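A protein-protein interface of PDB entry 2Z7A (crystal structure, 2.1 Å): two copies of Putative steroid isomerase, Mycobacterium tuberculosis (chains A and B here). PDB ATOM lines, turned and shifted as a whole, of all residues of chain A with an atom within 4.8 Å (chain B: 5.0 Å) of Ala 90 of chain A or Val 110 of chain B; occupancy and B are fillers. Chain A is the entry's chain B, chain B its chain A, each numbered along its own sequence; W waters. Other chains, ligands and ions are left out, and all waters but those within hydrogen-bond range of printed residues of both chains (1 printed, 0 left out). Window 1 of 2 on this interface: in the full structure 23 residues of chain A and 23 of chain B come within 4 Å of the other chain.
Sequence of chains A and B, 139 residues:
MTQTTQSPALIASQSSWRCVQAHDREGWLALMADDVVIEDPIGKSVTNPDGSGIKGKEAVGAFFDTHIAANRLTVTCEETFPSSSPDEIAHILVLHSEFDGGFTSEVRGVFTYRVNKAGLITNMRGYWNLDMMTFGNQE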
ATOM      1  N   GLU A  79      21.235  21.077   0.278  1.00  0.00           N
ATOM      2  CA  GLU A  79      21.449  21.341   1.651  1.00  0.00           C
ATOM      3  C   GLU A  79      21.262  22.852   1.908  1.00  0.00           C
ATOM      4  O   GLU A  79      21.620  23.699   1.097  1.00  0.00           O
ATOM      5  CB  GLU A  79      22.859  20.848   2.097  1.00  0.00           C
ATOM      6  CG  GLU A  79      23.000  20.753   3.621  1.00  0.00           C
ATOM      7  CD  GLU A  79      24.195  19.975   4.132  1.00  0.00           C
ATOM      8  OE1 GLU A  79      25.066  19.521   3.341  1.00  0.00           O
ATOM      9  OE2 GLU A  79      24.254  19.832   5.360  1.00  0.00           O
ATOM     10  N   THR A  80      20.689  23.136   3.071  1.00  0.00           N
ATOM     11  CA  THR A  80      20.517  24.491   3.613  1.00  0.00           C
ATOM     12  C   THR A  80      21.370  24.742   4.808  1.00  0.00           C
ATOM     13  O   THR A  80      21.389  23.931   5.723  1.00  0.00           O
ATOM     14  CB  THR A  80      19.012  24.767   3.959  1.00  0.00           C
ATOM     15  OG1 THR A  80      18.225  24.600   2.742  1.00  0.00           O
ATOM     16  CG2 THR A  80      18.833  26.192   4.534  1.00  0.00           C
ATOM     17  N   PHE A  81      22.028  25.913   4.816  1.00  0.00           N
ATOM     18  CA  PHE A  81      22.864  26.362   5.944  1.00  0.00           C
ATOM     19  C   PHE A  81      22.373  27.689   6.536  1.00  0.00           C
ATOM     20  O   PHE A  81      22.745  28.749   6.029  1.00  0.00           O
ATOM     21  CB  PHE A  81      24.321  26.514   5.442  1.00  0.00           C
ATOM     22  CG  PHE A  81      24.968  25.173   5.067  1.00  0.00           C
ATOM     23  CD1 PHE A  81      25.707  24.448   6.019  1.00  0.00           C
ATOM     24  CD2 PHE A  81      24.831  24.647   3.780  1.00  0.00           C
ATOM     25  CE1 PHE A  81      26.323  23.199   5.662  1.00  0.00           C
ATOM     26  CE2 PHE A  81      25.393  23.393   3.427  1.00  0.00           C
ATOM     27  CZ  PHE A  81      26.133  22.669   4.366  1.00  0.00           C
ATOM     28  N   GLU A  88      19.792  36.093   6.459  1.00  0.00           N
ATOM     29  CA  GLU A  88      20.826  35.641   5.514  1.00  0.00           C
ATOM     30  C   GLU A  88      20.985  34.159   5.584  1.00  0.00           C
ATOM     31  O   GLU A  88      21.012  33.607   6.663  1.00  0.00           O
ATOM     32  CB  GLU A  88      22.171  36.313   5.767  1.00  0.00           C
ATOM     33  CG  GLU A  88      22.208  37.817   5.623  1.00  0.00           C
ATOM     34  CD  GLU A  88      23.579  38.371   5.269  1.00  0.00           C
ATOM     35  OE1 GLU A  88      24.253  37.878   4.333  1.00  0.00           O
ATOM     36  OE2 GLU A  88      24.012  39.301   5.924  1.00  0.00           O
ATOM     37  N   ILE A  89      21.103  33.489   4.430  1.00  0.00           N
ATOM     38  CA  ILE A  89      21.071  32.032   4.382  1.00  0.00           C
ATOM     39  C   ILE A  89      21.903  31.571   3.187  1.00  0.00           C
ATOM     40  O   ILE A  89      22.098  32.332   2.253  1.00  0.00           O
ATOM     41  CB  ILE A  89      19.564  31.475   4.296  1.00  0.00           C
ATOM     42  CG1 ILE A  89      19.466  29.981   4.618  1.00  0.00           C
ATOM     43  CG2 ILE A  89      18.869  31.809   2.834  1.00  0.00           C
ATOM     44  CD1 ILE A  89      18.071  29.572   5.073  1.00  0.00           C
ATOM     45  N   ALA A  90      22.454  30.350   3.270  1.00  0.00           N
ATOM     46  CA  ALA A  90      23.232  29.735   2.173  1.00  0.00           C
ATOM     47  C   ALA A  90      22.656  28.357   1.860  1.00  0.00           C
ATOM     48  O   ALA A  90      22.087  27.678   2.730  1.00  0.00           O
ATOM     49  CB  ALA A  90      24.713  29.607   2.552  1.00  0.00           C
ATOM     50  N   HIS A  91      22.710  27.984   0.585  1.00  0.00           N
ATOM     51  CA  HIS A  91      22.227  26.666   0.181  1.00  0.00           C
ATOM     52  C   HIS A  91      23.221  26.019  -0.784  1.00  0.00           C
ATOM     53  O   HIS A  91      23.863  26.699  -1.590  1.00  0.00           O
ATOM     54  CB  HIS A  91      20.832  26.714  -0.528  1.00  0.00           C
ATOM     55  CG  HIS A  91      19.778  27.548   0.159  1.00  0.00           C
ATOM     56  ND1 HIS A  91      18.883  27.041   1.070  1.00  0.00           N
ATOM     57  CD2 HIS A  91      19.435  28.851  -0.013  1.00  0.00           C
ATOM     58  CE1 HIS A  91      18.048  27.995   1.451  1.00  0.00           C
ATOM     59  NE2 HIS A  91      18.357  29.101   0.793  1.00  0.00           N
ATOM     60  N   ILE A  92      23.303  24.695  -0.760  1.00  0.00           N
ATOM     61  CA  ILE A  92      23.883  23.982  -1.920  1.00  0.00           C
ATOM     62  C   ILE A  92      22.695  23.667  -2.839  1.00  0.00           C
ATOM     63  O   ILE A  92      21.762  23.052  -2.409  1.00  0.00           O
ATOM     64  CB  ILE A  92      24.651  22.663  -1.507  1.00  0.00           C
ATOM     65  CG1 ILE A  92      25.932  23.034  -0.781  1.00  0.00           C
ATOM     66  CG2 ILE A  92      25.004  21.819  -2.716  1.00  0.00           C
ATOM     67  CD1 ILE A  92      26.393  21.965   0.132  1.00  0.00           C
ATOM     68  N   VAL A 110      27.132  26.801  -4.518  1.00  0.00           N
ATOM     69  CA  VAL A 110      26.653  27.431  -3.274  1.00  0.00           C
ATOM     70  C   VAL A 110      25.988  28.748  -3.681  1.00  0.00           C
ATOM     71  O   VAL A 110      26.520  29.495  -4.452  1.00  0.00           O
ATOM     72  CB  VAL A 110      27.791  27.688  -2.256  1.00  0.00           C
ATOM     73  CG1 VAL A 110      27.334  28.720  -1.154  1.00  0.00           C
ATOM     74  CG2 VAL A 110      28.114  26.387  -1.578  1.00  0.00           C
ATOM     75  N   PHE A 111      24.807  28.971  -3.152  1.00  0.00           N
ATOM     76  CA  PHE A 111      23.980  30.181  -3.425  1.00  0.00           C
ATOM     77  C   PHE A 111      23.670  30.879  -2.110  1.00  0.00           C
ATOM     78  O   PHE A 111      23.158  30.258  -1.190  1.00  0.00           O
ATOM     79  CB  PHE A 111      22.710  29.787  -4.159  1.00  0.00           C
ATOM     80  CG  PHE A 111      22.999  29.275  -5.572  1.00  0.00           C
ATOM     81  CD1 PHE A 111      22.972  30.109  -6.639  1.00  0.00           C
ATOM     82  CD2 PHE A 111      23.410  27.920  -5.754  1.00  0.00           C
ATOM     83  CE1 PHE A 111      23.281  29.632  -7.891  1.00  0.00           C
ATOM     84  CE2 PHE A 111      23.725  27.415  -6.984  1.00  0.00           C
ATOM     85  CZ  PHE A 111      23.647  28.249  -8.057  1.00  0.00           C
ATOM     86  N   THR A 112      24.025  32.155  -2.015  1.00  0.00           N
ATOM     87  CA  THR A 112      23.714  32.839  -0.800  1.00  0.00           C
ATOM     88  C   THR A 112      22.581  33.863  -1.061  1.00  0.00           C
ATOM     89  O   THR A 112      22.491  34.420  -2.127  1.00  0.00           O
ATOM     90  CB  THR A 112      24.952  33.495  -0.145  1.00  0.00           C
ATOM     91  OG1 THR A 112      25.494  34.496  -1.037  1.00  0.00           O
ATOM     92  CG2 THR A 112      26.109  32.513   0.135  1.00  0.00           C
ATOM     93  N   ALA B  90      33.596  30.042  -1.913  1.00  0.00           N
ATOM     94  CA  ALA B  90      32.861  29.469  -0.802  1.00  0.00           C
ATOM     95  C   ALA B  90      33.416  28.075  -0.469  1.00  0.00           C
ATOM     96  O   ALA B  90      33.937  27.390  -1.357  1.00  0.00           O
ATOM     97  CB  ALA B  90      31.409  29.348  -1.113  1.00  0.00           C
ATOM     98  N   HIS B  91      33.306  27.658   0.804  1.00  0.00           N
ATOM     99  CA  HIS B  91      33.701  26.321   1.203  1.00  0.00           C
ATOM    100  C   HIS B  91      32.708  25.791   2.146  1.00  0.00           C
ATOM    101  O   HIS B  91      32.000  26.563   2.790  1.00  0.00           O
ATOM    102  CB  HIS B  91      35.084  26.267   1.919  1.00  0.00           C
ATOM    103  CG  HIS B  91      36.162  27.013   1.240  1.00  0.00           C
ATOM    104  ND1 HIS B  91      37.084  26.413   0.413  1.00  0.00           N
ATOM    105  CD2 HIS B  91      36.490  28.328   1.285  1.00  0.00           C
ATOM    106  CE1 HIS B  91      37.948  27.316  -0.013  1.00  0.00           C
ATOM    107  NE2 HIS B  91      37.600  28.491   0.495  1.00  0.00           N
ATOM    108  N   ILE B  92      32.668  24.459   2.293  1.00  0.00           N
ATOM    109  CA  ILE B  92      31.919  23.828   3.420  1.00  0.00           C
ATOM    110  C   ILE B  92      33.035  23.406   4.371  1.00  0.00           C
ATOM    111  O   ILE B  92      33.881  22.557   4.007  1.00  0.00           O
ATOM    112  CB  ILE B  92      31.034  22.598   2.952  1.00  0.00           C
ATOM    113  CG1 ILE B  92      30.085  22.926   1.749  1.00  0.00           C
ATOM    114  CG2 ILE B  92      30.372  21.821   4.128  1.00  0.00           C
ATOM    115  CD1 ILE B  92      29.109  24.079   1.914  1.00  0.00           C
ATOM    116  N   ARG B 108      29.568  22.595  11.530  1.00  0.00           N
ATOM    117  CA  ARG B 108      29.759  22.501  10.085  1.00  0.00           C
ATOM    118  C   ARG B 108      28.960  23.589   9.372  1.00  0.00           C
ATOM    119  O   ARG B 108      27.771  23.692   9.588  1.00  0.00           O
ATOM    120  CB  ARG B 108      29.242  21.146   9.613  1.00  0.00           C
ATOM    121  CG  ARG B 108      29.391  20.929   8.083  1.00  0.00           C
ATOM    122  CD  ARG B 108      29.120  19.367   7.767  1.00  0.00           C
ATOM    123  NE  ARG B 108      28.895  19.121   6.329  1.00  0.00           N
ATOM    124  CZ  ARG B 108      27.743  19.311   5.700  1.00  0.00           C
ATOM    125  NH1 ARG B 108      26.636  19.724   6.363  1.00  0.00           N
ATOM    126  NH2 ARG B 108      27.695  19.041   4.419  1.00  0.00           N
ATOM    127  N   GLY B 109      29.586  24.354   8.470  1.00  0.00           N
ATOM    128  CA  GLY B 109      28.837  25.393   7.789  1.00  0.00           C
ATOM    129  C   GLY B 109      29.481  25.817   6.491  1.00  0.00           C
ATOM    130  O   GLY B 109      30.567  25.341   6.151  1.00  0.00           O
ATOM    131  N   VAL B 110      28.802  26.753   5.816  1.00  0.00           N
ATOM    132  CA  VAL B 110      29.324  27.456   4.687  1.00  0.00           C
ATOM    133  C   VAL B 110      30.132  28.694   5.128  1.00  0.00           C
ATOM    134  O   VAL B 110      29.675  29.490   5.960  1.00  0.00           O
ATOM    135  CB  VAL B 110      28.156  27.831   3.685  1.00  0.00           C
ATOM    136  CG1 VAL B 110      28.565  28.875   2.666  1.00  0.00           C
ATOM    137  CG2 VAL B 110      27.633  26.570   3.014  1.00  0.00           C
ATOM    138  N   PHE B 111      31.285  28.895   4.490  1.00  0.00           N
ATOM    139  CA  PHE B 111      32.161  30.041   4.746  1.00  0.00           C
ATOM    140  C   PHE B 111      32.506  30.622   3.446  1.00  0.00           C
ATOM    141  O   PHE B 111      32.948  29.894   2.544  1.00  0.00           O
ATOM    142  CB  PHE B 111      33.405  29.568   5.544  1.00  0.00           C
ATOM    143  CG  PHE B 111      33.031  29.096   6.962  1.00  0.00           C
ATOM    144  CD1 PHE B 111      33.119  29.954   8.048  1.00  0.00           C
ATOM    145  CD2 PHE B 111      32.527  27.828   7.180  1.00  0.00           C
ATOM    146  CE1 PHE B 111      32.769  29.528   9.303  1.00  0.00           C
ATOM    147  CE2 PHE B 111      32.138  27.416   8.474  1.00  0.00           C
ATOM    148  CZ  PHE B 111      32.252  28.272   9.516  1.00  0.00           C
ATOM    149  N   THR B 112      32.220  31.915   3.287  1.00  0.00           N
ATOM    150  CA  THR B 112      32.626  32.669   2.075  1.00  0.00           C
ATOM    151  C   THR B 112      33.792  33.610   2.300  1.00  0.00           C
ATOM    152  O   THR B 112      33.926  34.177   3.383  1.00  0.00           O
ATOM    153  CB  THR B 112      31.428  33.441   1.456  1.00  0.00           C
ATOM    154  OG1 THR B 112      30.988  34.480   2.342  1.00  0.00           O
ATOM    155  CG2 THR B 112      30.193  32.436   1.210  1.00  0.00           C
ATOM    156  N   ARG B 125      32.807  35.176   5.940  1.00  0.00           N
ATOM    157  CA  ARG B 125      31.472  35.093   6.474  1.00  0.00           C
ATOM    158  C   ARG B 125      31.037  33.681   6.660  1.00  0.00           C
ATOM    159  O   ARG B 125      31.159  32.894   5.769  1.00  0.00           O
ATOM    160  CB  ARG B 125      30.495  35.789   5.489  1.00  0.00           C
ATOM    161  CG  ARG B 125      31.079  37.085   4.957  1.00  0.00           C
ATOM    162  CD  ARG B 125      30.091  38.028   4.213  1.00  0.00           C
ATOM    163  NE  ARG B 125      29.066  38.650   5.093  1.00  0.00           N
ATOM    164  CZ  ARG B 125      27.758  38.576   4.897  1.00  0.00           C
ATOM    165  NH1 ARG B 125      27.244  37.910   3.821  1.00  0.00           N
ATOM    166  NH2 ARG B 125      26.956  39.224   5.738  1.00  0.00           N
ATOM    167  N   GLY B 126      30.479  33.361   7.825  1.00  0.00           N
ATOM    168  CA  GLY B 126      30.095  32.010   8.102  1.00  0.00           C
ATOM    169  C   GLY B 126      28.634  31.864   8.316  1.00  0.00           C
ATOM    170  O   GLY B 126      28.001  32.630   9.062  1.00  0.00           O
ATOM    171  N   TYR B 127      28.087  30.819   7.691  1.00  0.00           N
ATOM    172  CA  TYR B 127      26.682  30.482   7.799  1.00  0.00           C
ATOM    173  C   TYR B 127      26.612  29.314   8.799  1.00  0.00           C
ATOM    174  O   TYR B 127      26.722  28.132   8.404  1.00  0.00           O
ATOM    175  CB  TYR B 127      26.085  30.105   6.377  1.00  0.00           C
ATOM    176  CG  TYR B 127      26.046  31.296   5.418  1.00  0.00           C
ATOM    177  CD1 TYR B 127      24.868  32.038   5.214  1.00  0.00           C
ATOM    178  CD2 TYR B 127      27.154  31.681   4.738  1.00  0.00           C
ATOM    179  CE1 TYR B 127      24.894  33.166   4.349  1.00  0.00           C
ATOM    180  CE2 TYR B 127      27.166  32.747   3.885  1.00  0.00           C
ATOM    181  CZ  TYR B 127      26.000  33.489   3.704  1.00  0.00           C
ATOM    182  OH  TYR B 127      26.020  34.565   2.873  1.00  0.00           O
HETATM  183  O   HOH W   1      23.806  36.041   2.521  1.00  0.00           O
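Water W1 bridges OE1 of Glu 88 of chain A (2.6 Å) and OH of Tyr 127 of chain B (2.7 Å).
N of Tyr 127 of chain B sits at hydrogen-bond distance from O of Val 110 of chain B, at 2.7 Å.
The backbone NH of Ile 92 of chain A sits at hydrogen-bond distance from the backbone carbonyl oxygen of Glu 79 of chain A, 2.7 Å away.
The backbone NH (N) of Phe 81 of chain A lies within hydrogen-bond range of the backbone carbonyl oxygen (O) of Ala 90 of chain A (2.7 Å).
The backbone NH of Thr 112 of chain B lies within hydrogen-bond range of the backbone carbonyl oxygen of Arg 125 of chain B (2.9 Å).
Of chain B, only Val 110 and Tyr 127 come within 4 Å of Ala 90 of chain A.
Printed residues of chain A within 4 Å of Val 110 of chain B: Phe 81 (3.5 Å) and Ala 90 (3.9 Å).
Of the printed residues of chain A, Arg 125 of chain B touches Glu 88.
Printed residues of chain A within 4 Å of Arg 108 of chain B: Glu 79 and Phe 81.
Of the printed residues of chain A, Ile 92 of chain B touches Ile 92.
Of the printed residues of chain B, Thr 112 of chain A touches Tyr 127 (3.4 Å).
His 91 of chain B touches none of the printed residues of chain A.
The nearest printed residue of chain B that does not touch Ala 90 of chain A is Thr 112 of chain B (6.3 Å).
The nearest printed residue of chain B that does not touch Ile 92 of chain A is Arg 108 of chain B (5.4 Å).
Ala 90 of chain A touches Val 110 of chain B, but with the chains exchanged Val 110 of chain A does not touch Ala 90 of chain B (4.1 Å).
Ile 92 of chain B touches its own counterpart, Ile 92 of chain A.
6 positions are printed for both chains.
Of the 11 pairs that touch across the chains among the printed residues, 1 has its exchanged pair printed and touching as well.
The guanidinium group (NH1) of Arg 108 of chain B lies within salt-bridge range of the side-chain carboxylate (OE2) of Glu 79 of chain A (2.6 Å).
The guanidinium group of Arg 125 of chain B lies within salt-bridge range of the side-chain carboxylate of Glu 88 of chain A.
Hydrophobic or aromatic side chains of chain A that line the printed part of chain B: Phe 81, Ala 90 and Ile 92.
Of the 11 printed residues of chain B, 6 touch a printed residue of chain A.
Hydrophobic or aromatic side chains of chain B that line the printed part of chain A: Ile 92, Val 110 and Tyr 127.
Among the printed residues, 11 pairs touch across the chains.
Among the printed residues, pairs that only touch across the chains: Phe 81 of chain A with Arg 108 of chain B, Phe 81 of chain A with Gly 109 of chain B, Phe 81 of chain A with Val 110 of chain B, Phe 81 of chain A with Tyr 127 of chain B, Ile 89 of chain A with Tyr 127 of chain B, Ala 90 of chain A with Val 110 of chain B, Ala 90 of chain A with Tyr 127 of chain B, Ile 92 of chain A with Ile 92 of chain B and Thr 112 of chain A with Tyr 127 of chain B.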
